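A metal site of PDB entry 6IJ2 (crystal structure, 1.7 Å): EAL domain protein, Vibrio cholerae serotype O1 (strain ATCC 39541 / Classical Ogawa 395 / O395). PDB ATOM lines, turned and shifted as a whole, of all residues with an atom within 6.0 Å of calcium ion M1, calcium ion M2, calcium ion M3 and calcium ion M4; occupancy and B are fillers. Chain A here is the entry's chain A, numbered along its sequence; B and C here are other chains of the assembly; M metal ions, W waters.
The side-chain carboxylate (OD1) of Asp 181 is in hydrogen-bond range of the side-chain hydroxyl (OG) of Ser 162, at 3.2 Å.
OE1 of Glu 128 lies within salt-bridge range of NZ of Lys 179.
The side-chain amino group of Lys 179 sits close to the side-chain carboxylate of Glu 215 (3.5 Å).
N of Glu 215 is in hydrogen-bond range of O of Val 180 (3.0 Å).
O2' of G 2 of chain B sits close to OD1 of Asn 95, 3.4 Å away.
The side-chain carboxylate of Glu 45 lies within salt-bridge range of the side-chain amino group of Lys 179, at 3.3 Å.
Of the 23 residues printed, 5 come within 4 Å of calcium ion M1.
Of the 23 residues printed, 4 come within 4 Å of calcium ion M2.
Three residues have an atom within 4 Å of calcium ion M3: Asp 159, Ser 162 and Tyr 164.
Four residues have an atom within 4 Å of calcium ion M4: Thr 130, Asp 158, Asp 159 and G 1 of chain B.
Calcium ion M1 is bound by the side-chain carboxylate (OE2) of Glu 128, water W1, the side-chain amide oxygen (OD1) of Asn 95, the side-chain carboxylate (OE2) of Glu 45, the side-chain carboxylate (OD2) of Asp 158, OP1 of G 1 of chain B and the side-chain carboxylate (OD1) of Asp 158.
Calcium ion M1 has seven donor atoms within binding distance.
Calcium ion M2 is bound by water W4 (2.3 Å), OD1 of Asp 158 (2.3 Å), OP3 of G 1 of chain B (2.3 Å), OE2 of Glu 215 (2.3 Å), O of Asp 158 (2.4 Å), OD1 of Asp 159 (2.4 Å) and OE1 of Glu 215 (2.5 Å).
Calcium ion M3 is bound by the backbone carbonyl oxygen of Ser 162 (2.2 Å), the backbone carbonyl oxygen of Tyr 164 (2.2 Å), water W5 (2.4 Å), the backbone carbonyl oxygen of Asp 159 (2.4 Å) and water W3 (2.5 Å).
Calcium ion M3 has five donor atoms within binding distance.
Calcium ion M4 is bound by water W2, the side-chain carboxylate (OD2) of Asp 159, OP2 of G 1 of chain B, the side-chain hydroxyl (OG1) of Thr 130 and the side-chain carboxylate (OD1) of Asp 159.
Calcium ion M4 has five donor atoms within binding distance.
Water W1 lies within hydrogen-bond range of the side-chain carboxylate (OE1) of Glu 45 (2.7 Å) and the side-chain amino group (NZ) of Lys 179 (3.0 Å).
Water W3 lies within hydrogen-bond range of OE1 of Glu 131 (2.7 Å) and N of Tyr 164 (3.0 Å).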
ATOM      1  N   GLU A  45       1.096 -39.529  24.797  1.00  0.00           N
ATOM      2  CA  GLU A  45       0.537 -38.416  24.065  1.00  0.00           C
ATOM      3  C   GLU A  45       1.311 -38.253  22.756  1.00  0.00           C
ATOM      4  O   GLU A  45       2.555 -38.280  22.760  1.00  0.00           O
ATOM      5  CB  GLU A  45       0.587 -37.124  24.880  1.00  0.00           C
ATOM      6  CG  GLU A  45       0.024 -35.957  24.111  1.00  0.00           C
ATOM      7  CD  GLU A  45       0.056 -34.647  24.865  1.00  0.00           C
ATOM      8  OE1 GLU A  45       0.688 -34.560  25.946  1.00  0.00           O
ATOM      9  OE2 GLU A  45      -0.572 -33.700  24.342  1.00  0.00           O
ATOM     10  N   LEU A  47       2.547 -36.001  19.693  1.00  0.00           N
ATOM     11  CA  LEU A  47       2.923 -34.595  19.569  1.00  0.00           C
ATOM     12  C   LEU A  47       3.535 -34.363  18.200  1.00  0.00           C
ATOM     13  O   LEU A  47       4.452 -35.089  17.801  1.00  0.00           O
ATOM     14  CB  LEU A  47       3.915 -34.196  20.652  1.00  0.00           C
ATOM     15  CG  LEU A  47       3.381 -34.325  22.082  1.00  0.00           C
ATOM     16  CD1 LEU A  47       4.550 -34.355  23.034  1.00  0.00           C
ATOM     17  CD2 LEU A  47       2.449 -33.158  22.411  1.00  0.00           C
ATOM     18  N   ASN A  95      -4.102 -34.658  20.564  1.00  0.00           N
ATOM     19  CA  ASN A  95      -4.542 -33.287  20.809  1.00  0.00           C
ATOM     20  C   ASN A  95      -5.575 -32.899  19.755  1.00  0.00           C
ATOM     21  O   ASN A  95      -5.345 -33.067  18.554  1.00  0.00           O
ATOM     22  CB  ASN A  95      -3.354 -32.329  20.744  1.00  0.00           C
ATOM     23  CG  ASN A  95      -2.434 -32.464  21.935  1.00  0.00           C
ATOM     24  OD1 ASN A  95      -2.718 -31.969  23.020  1.00  0.00           O
ATOM     25  ND2 ASN A  95      -1.312 -33.153  21.737  1.00  0.00           N
ATOM     26  N   GLU A 128      -7.621 -35.042  23.664  1.00  0.00           N
ATOM     27  CA  GLU A 128      -7.399 -33.958  24.613  1.00  0.00           C
ATOM     28  C   GLU A 128      -7.950 -32.660  24.030  1.00  0.00           C
ATOM     29  O   GLU A 128      -7.603 -32.284  22.904  1.00  0.00           O
ATOM     30  CB  GLU A 128      -5.916 -33.805  24.937  1.00  0.00           C
ATOM     31  CG  GLU A 128      -5.281 -35.116  25.350  1.00  0.00           C
ATOM     32  CD  GLU A 128      -3.856 -34.959  25.813  1.00  0.00           C
ATOM     33  OE1 GLU A 128      -3.268 -35.970  26.231  1.00  0.00           O
ATOM     34  OE2 GLU A 128      -3.320 -33.821  25.781  1.00  0.00           O
ATOM     35  N   THR A 130      -8.655 -28.649  23.979  1.00  0.00           N
ATOM     36  CA  THR A 130      -8.263 -27.286  24.294  1.00  0.00           C
ATOM     37  C   THR A 130      -9.232 -26.340  23.588  1.00  0.00           C
ATOM     38  O   THR A 130      -9.578 -26.543  22.416  1.00  0.00           O
ATOM     39  CB  THR A 130      -6.831 -26.969  23.826  1.00  0.00           C
ATOM     40  OG1 THR A 130      -5.905 -27.878  24.439  1.00  0.00           O
ATOM     41  CG2 THR A 130      -6.452 -25.543  24.203  1.00  0.00           C
ATOM     42  N   GLU A 131      -9.656 -25.307  24.302  1.00  0.00           N
ATOM     43  CA  GLU A 131     -10.572 -24.318  23.739  1.00  0.00           C
ATOM     44  C   GLU A 131      -9.852 -23.416  22.741  1.00  0.00           C
ATOM     45  O   GLU A 131      -8.665 -23.108  22.899  1.00  0.00           O
ATOM     46  CB  GLU A 131     -11.184 -23.480  24.854  1.00  0.00           C
ATOM     47  CG  GLU A 131     -11.717 -24.297  26.033  1.00  0.00           C
ATOM     48  CD  GLU A 131     -10.691 -24.486  27.152  1.00  0.00           C
ATOM     49  OE1 GLU A 131      -9.543 -24.874  26.845  1.00  0.00           O
ATOM     50  OE2 GLU A 131     -11.039 -24.234  28.326  1.00  0.00           O
ATOM     51  N   ILE A 157      -9.835 -32.967  29.385  1.00  0.00           N
ATOM     52  CA  ILE A 157      -9.568 -31.533  29.346  1.00  0.00           C
ATOM     53  C   ILE A 157      -8.062 -31.349  29.448  1.00  0.00           C
ATOM     54  O   ILE A 157      -7.424 -31.808  30.392  1.00  0.00           O
ATOM     55  CB  ILE A 157     -10.314 -30.795  30.478  1.00  0.00           C
ATOM     56  CG1 ILE A 157     -11.815 -30.895  30.244  1.00  0.00           C
ATOM     57  CG2 ILE A 157      -9.864 -29.339  30.545  1.00  0.00           C
ATOM     58  CD1 ILE A 157     -12.629 -30.269  31.314  1.00  0.00           C
ATOM     59  N   ASP A 158      -7.478 -30.697  28.438  1.00  0.00           N
ATOM     60  CA  ASP A 158      -6.017 -30.645  28.316  1.00  0.00           C
ATOM     61  C   ASP A 158      -5.388 -29.624  29.269  1.00  0.00           C
ATOM     62  O   ASP A 158      -4.340 -29.880  29.877  1.00  0.00           O
ATOM     63  CB  ASP A 158      -5.675 -30.324  26.860  1.00  0.00           C
ATOM     64  CG  ASP A 158      -4.230 -30.613  26.483  1.00  0.00           C
ATOM     65  OD1 ASP A 158      -3.396 -30.949  27.355  1.00  0.00           O
ATOM     66  OD2 ASP A 158      -3.933 -30.533  25.281  1.00  0.00           O
ATOM     67  N   ASP A 159      -5.989 -28.469  29.422  1.00  0.00           N
ATOM     68  CA  ASP A 159      -5.211 -27.373  29.978  1.00  0.00           C
ATOM     69  C   ASP A 159      -5.910 -26.817  31.198  1.00  0.00           C
ATOM     70  O   ASP A 159      -6.143 -25.612  31.287  1.00  0.00           O
ATOM     71  CB  ASP A 159      -4.976 -26.277  28.942  1.00  0.00           C
ATOM     72  CG  ASP A 159      -4.278 -26.796  27.671  1.00  0.00           C
ATOM     73  OD1 ASP A 159      -3.680 -27.889  27.688  1.00  0.00           O
ATOM     74  OD2 ASP A 159      -4.313 -26.062  26.644  1.00  0.00           O
ATOM     75  N   PHE A 160      -6.247 -27.665  32.158  1.00  0.00           N
ATOM     76  CA  PHE A 160      -6.855 -27.158  33.389  1.00  0.00           C
ATOM     77  C   PHE A 160      -5.836 -26.353  34.194  1.00  0.00           C
ATOM     78  O   PHE A 160      -4.763 -26.838  34.537  1.00  0.00           O
ATOM     79  CB  PHE A 160      -7.389 -28.291  34.237  1.00  0.00           C
ATOM     80  CG  PHE A 160      -8.181 -27.826  35.420  1.00  0.00           C
ATOM     81  CD1 PHE A 160      -9.539 -27.606  35.309  1.00  0.00           C
ATOM     82  CD2 PHE A 160      -7.568 -27.616  36.635  1.00  0.00           C
ATOM     83  CE1 PHE A 160     -10.281 -27.191  36.398  1.00  0.00           C
ATOM     84  CE2 PHE A 160      -8.291 -27.181  37.734  1.00  0.00           C
ATOM     85  CZ  PHE A 160      -9.646 -26.977  37.608  1.00  0.00           C
ATOM     86  N   GLY A 161      -6.201 -25.135  34.541  1.00  0.00           N
ATOM     87  CA  GLY A 161      -5.315 -24.282  35.294  1.00  0.00           C
ATOM     88  C   GLY A 161      -4.478 -23.333  34.474  1.00  0.00           C
ATOM     89  O   GLY A 161      -3.614 -22.656  35.047  1.00  0.00           O
ATOM     90  N   SER A 162      -4.702 -23.253  33.173  1.00  0.00           N
ATOM     91  CA  SER A 162      -4.078 -22.235  32.345  1.00  0.00           C
ATOM     92  C   SER A 162      -5.027 -21.840  31.225  1.00  0.00           C
ATOM     93  O   SER A 162      -6.069 -22.462  31.033  1.00  0.00           O
ATOM     94  CB  SER A 162      -2.759 -22.728  31.748  1.00  0.00           C
ATOM     95  OG  SER A 162      -3.019 -23.774  30.835  1.00  0.00           O
ATOM     96  N   GLY A 163      -4.664 -20.815  30.479  1.00  0.00           N
ATOM     97  CA  GLY A 163      -5.449 -20.475  29.307  1.00  0.00           C
ATOM     98  C   GLY A 163      -6.878 -20.065  29.642  1.00  0.00           C
ATOM     99  O   GLY A 163      -7.109 -19.120  30.416  1.00  0.00           O
ATOM    100  N   TYR A 164      -7.844 -20.772  29.072  1.00  0.00           N
ATOM    101  CA  TYR A 164      -9.258 -20.515  29.295  1.00  0.00           C
ATOM    102  C   TYR A 164      -9.752 -21.262  30.526  1.00  0.00           C
ATOM    103  O   TYR A 164      -9.124 -22.203  30.997  1.00  0.00           O
ATOM    104  CB  TYR A 164     -10.044 -20.897  28.043  1.00  0.00           C
ATOM    105  CG  TYR A 164      -9.577 -20.087  26.838  1.00  0.00           C
ATOM    106  CD1 TYR A 164      -9.896 -18.752  26.729  1.00  0.00           C
ATOM    107  CD2 TYR A 164      -8.790 -20.664  25.842  1.00  0.00           C
ATOM    108  CE1 TYR A 164      -9.472 -17.995  25.648  1.00  0.00           C
ATOM    109  CE2 TYR A 164      -8.364 -19.914  24.749  1.00  0.00           C
ATOM    110  CZ  TYR A 164      -8.696 -18.576  24.660  1.00  0.00           C
ATOM    111  OH  TYR A 164      -8.285 -17.823  23.586  1.00  0.00           O
ATOM    112  N   SER A 165     -10.896 -20.821  31.065  1.00  0.00           N
ATOM    113  CA  SER A 165     -11.382 -21.339  32.342  1.00  0.00           C
ATOM    114  C   SER A 165     -11.808 -22.793  32.205  1.00  0.00           C
ATOM    115  O   SER A 165     -12.787 -23.094  31.511  1.00  0.00           O
ATOM    116  CB  SER A 165     -12.550 -20.494  32.862  1.00  0.00           C
ATOM    117  OG  SER A 165     -13.141 -21.126  34.006  1.00  0.00           O
ATOM    118  N   GLY A 166     -11.079 -23.686  32.882  1.00  0.00           N
ATOM    119  CA  GLY A 166     -11.467 -25.084  32.910  1.00  0.00           C
ATOM    120  C   GLY A 166     -12.673 -25.352  33.780  1.00  0.00           C
ATOM    121  O   GLY A 166     -13.440 -26.265  33.511  1.00  0.00           O
ATOM    122  N   LYS A 179      -6.348 -33.017  32.648  1.00  0.00           N
ATOM    123  CA  LYS A 179      -4.908 -32.819  32.721  1.00  0.00           C
ATOM    124  C   LYS A 179      -4.633 -31.467  33.373  1.00  0.00           C
ATOM    125  O   LYS A 179      -5.190 -30.452  32.952  1.00  0.00           O
ATOM    126  CB  LYS A 179      -4.276 -32.861  31.327  1.00  0.00           C
ATOM    127  CG  LYS A 179      -4.502 -34.221  30.681  1.00  0.00           C
ATOM    128  CD  LYS A 179      -3.205 -34.856  30.160  1.00  0.00           C
ATOM    129  CE  LYS A 179      -2.807 -34.307  28.866  1.00  0.00           C
ATOM    130  NZ  LYS A 179      -1.588 -34.979  28.275  1.00  0.00           N
ATOM    131  N   VAL A 180      -3.785 -31.460  34.395  1.00  0.00           N
ATOM    132  CA  VAL A 180      -3.519 -30.241  35.162  1.00  0.00           C
ATOM    133  C   VAL A 180      -2.253 -29.611  34.628  1.00  0.00           C
ATOM    134  O   VAL A 180      -1.182 -30.229  34.627  1.00  0.00           O
ATOM    135  CB  VAL A 180      -3.404 -30.533  36.672  1.00  0.00           C
ATOM    136  CG1 VAL A 180      -3.087 -29.221  37.427  1.00  0.00           C
ATOM    137  CG2 VAL A 180      -4.695 -31.134  37.179  1.00  0.00           C
ATOM    138  N   ASP A 181      -2.371 -28.336  34.227  1.00  0.00           N
ATOM    139  CA  ASP A 181      -1.281 -27.615  33.594  1.00  0.00           C
ATOM    140  C   ASP A 181      -0.053 -27.593  34.499  1.00  0.00           C
ATOM    141  O   ASP A 181      -0.162 -27.483  35.715  1.00  0.00           O
ATOM    142  CB  ASP A 181      -1.723 -26.192  33.276  1.00  0.00           C
ATOM    143  CG  ASP A 181      -0.642 -25.399  32.579  1.00  0.00           C
ATOM    144  OD1 ASP A 181      -0.432 -25.621  31.378  1.00  0.00           O
ATOM    145  OD2 ASP A 181       0.000 -24.554  33.229  1.00  0.00           O
ATOM    146  N   GLU A 215       0.520 -32.729  34.547  1.00  0.00           N
ATOM    147  CA  GLU A 215       1.400 -32.437  33.420  1.00  0.00           C
ATOM    148  C   GLU A 215       2.688 -31.745  33.854  1.00  0.00           C
ATOM    149  O   GLU A 215       2.717 -30.989  34.828  1.00  0.00           O
ATOM    150  CB  GLU A 215       0.711 -31.553  32.383  1.00  0.00           C
ATOM    151  CG  GLU A 215      -0.536 -32.129  31.728  1.00  0.00           C
ATOM    152  CD  GLU A 215      -1.092 -31.218  30.640  1.00  0.00           C
ATOM    153  OE1 GLU A 215      -1.476 -31.733  29.581  1.00  0.00           O
ATOM    154  OE2 GLU A 215      -1.140 -29.974  30.820  1.00  0.00           O
ATOM    155  OP3   G B   1      -0.481 -29.368  27.260  1.00  0.00           O
ATOM    156  P     G B   1      -0.086 -29.105  25.902  1.00  0.00           P
ATOM    157  OP1   G B   1      -0.477 -30.166  25.035  1.00  0.00           O
ATOM    158  OP2   G B   1      -0.582 -27.800  25.610  1.00  0.00           O
ATOM    159  O5'   G B   1       1.481 -29.002  26.010  1.00  0.00           O
ATOM    160  C5'   G B   1       2.326 -30.049  25.544  1.00  0.00           C
ATOM    161  C4'   G B   1       3.751 -29.549  25.458  1.00  0.00           C
ATOM    162  O4'   G B   1       4.387 -29.685  26.744  1.00  0.00           O
ATOM    163  C3'   G B   1       4.670 -30.279  24.480  1.00  0.00           C
ATOM    164  O3'   G B   1       5.410 -29.408  23.647  1.00  0.00           O
ATOM    165  C2'   G B   1       5.638 -31.024  25.380  1.00  0.00           C
ATOM    166  O2'   G B   1       6.940 -31.174  24.893  1.00  0.00           O
ATOM    167  C1'   G B   1       5.702 -30.083  26.574  1.00  0.00           C
ATOM    168  N9    G B   1       6.157 -30.738  27.792  1.00  0.00           N
ATOM    169  C8    G B   1       5.891 -32.039  28.175  1.00  0.00           C
ATOM    170  N7    G B   1       6.413 -32.343  29.331  1.00  0.00           N
ATOM    171  C5    G B   1       7.047 -31.178  29.733  1.00  0.00           C
ATOM    172  C6    G B   1       7.789 -30.902  30.909  1.00  0.00           C
ATOM    173  O6    G B   1       8.046 -31.643  31.847  1.00  0.00           O
ATOM    174  N1    G B   1       8.273 -29.604  30.920  1.00  0.00           N
ATOM    175  C2    G B   1       8.055 -28.683  29.921  1.00  0.00           C
ATOM    176  N2    G B   1       8.575 -27.474  30.123  1.00  0.00           N
ATOM    177  N3    G B   1       7.357 -28.919  28.831  1.00  0.00           N
ATOM    178  C4    G B   1       6.886 -30.180  28.803  1.00  0.00           C
ATOM    179  P     G B   2       5.364 -29.551  22.134  1.00  0.00           P
ATOM    180  OP1   G B   2       5.418 -30.945  21.830  1.00  0.00           O
ATOM    181  OP2   G B   2       6.358 -28.673  21.609  1.00  0.00           O
ATOM    182  O5'   G B   2       3.953 -28.971  21.737  1.00  0.00           O
ATOM    183  C5'   G B   2       3.722 -27.571  21.645  1.00  0.00           C
ATOM    184  C4'   G B   2       2.247 -27.312  21.449  1.00  0.00           C
ATOM    185  O4'   G B   2       1.802 -27.978  20.253  1.00  0.00           O
ATOM    186  C3'   G B   2       1.341 -27.817  22.576  1.00  0.00           C
ATOM    187  O3'   G B   2       0.333 -26.875  22.900  1.00  0.00           O
ATOM    188  C2'   G B   2       0.660 -29.032  21.955  1.00  0.00           C
ATOM    189  O2'   G B   2      -0.623 -29.321  22.439  1.00  0.00           O
ATOM    190  C1'   G B   2       0.593 -28.616  20.496  1.00  0.00           C
ATOM    191  N9    G B   2       0.508 -29.792  19.638  1.00  0.00           N
ATOM    192  C8    G B   2       1.437 -30.784  19.517  1.00  0.00           C
ATOM    193  N7    G B   2       1.059 -31.742  18.729  1.00  0.00           N
ATOM    194  C5    G B   2      -0.213 -31.368  18.321  1.00  0.00           C
ATOM    195  C6    G B   2      -1.123 -32.011  17.462  1.00  0.00           C
ATOM    196  O6    G B   2      -1.011 -33.092  16.888  1.00  0.00           O
ATOM    197  N1    G B   2      -2.291 -31.281  17.322  1.00  0.00           N
ATOM    198  C2    G B   2      -2.556 -30.088  17.936  1.00  0.00           C
ATOM    199  N2    G B   2      -3.738 -29.544  17.678  1.00  0.00           N
ATOM    200  N3    G B   2      -1.703 -29.469  18.723  1.00  0.00           N
ATOM    201  C4    G B   2      -0.558 -30.161  18.872  1.00  0.00           C
ATOM    202  N   SER C 165      -8.624 -18.501  32.722  1.00  0.00           N
ATOM    203  CA  SER C 165      -8.477 -19.342  33.916  1.00  0.00           C
ATOM    204  C   SER C 165      -8.207 -18.495  35.160  1.00  0.00           C
ATOM    205  O   SER C 165      -7.151 -17.879  35.278  1.00  0.00           O
ATOM    206  CB  SER C 165      -7.356 -20.363  33.704  1.00  0.00           C
ATOM    207  OG  SER C 165      -7.033 -21.049  34.919  1.00  0.00           O
HETATM  208 CA    CA M   1      -2.022 -32.023  25.288  1.00  0.00          CA
HETATM  209 CA    CA M   2      -2.239 -29.526  28.800  1.00  0.00          CA
HETATM  210 CA    CA M   3      -7.724 -23.894  30.615  1.00  0.00          CA
HETATM  211 CA    CA M   4      -3.202 -27.478  24.960  1.00  0.00          CA
HETATM  212  O   HOH W   1      -0.592 -32.433  27.074  1.00  0.00           O
HETATM  213  O   HOH W   2      -2.783 -27.055  22.642  1.00  0.00           O
HETATM  214  O   HOH W   3      -7.507 -23.574  28.138  1.00  0.00           O
HETATM  215  O   HOH W   4      -1.829 -27.343  29.520  1.00  0.00           O
HETATM  216  O   HOH W   5      -9.397 -25.542  30.207  1.00  0.00           O
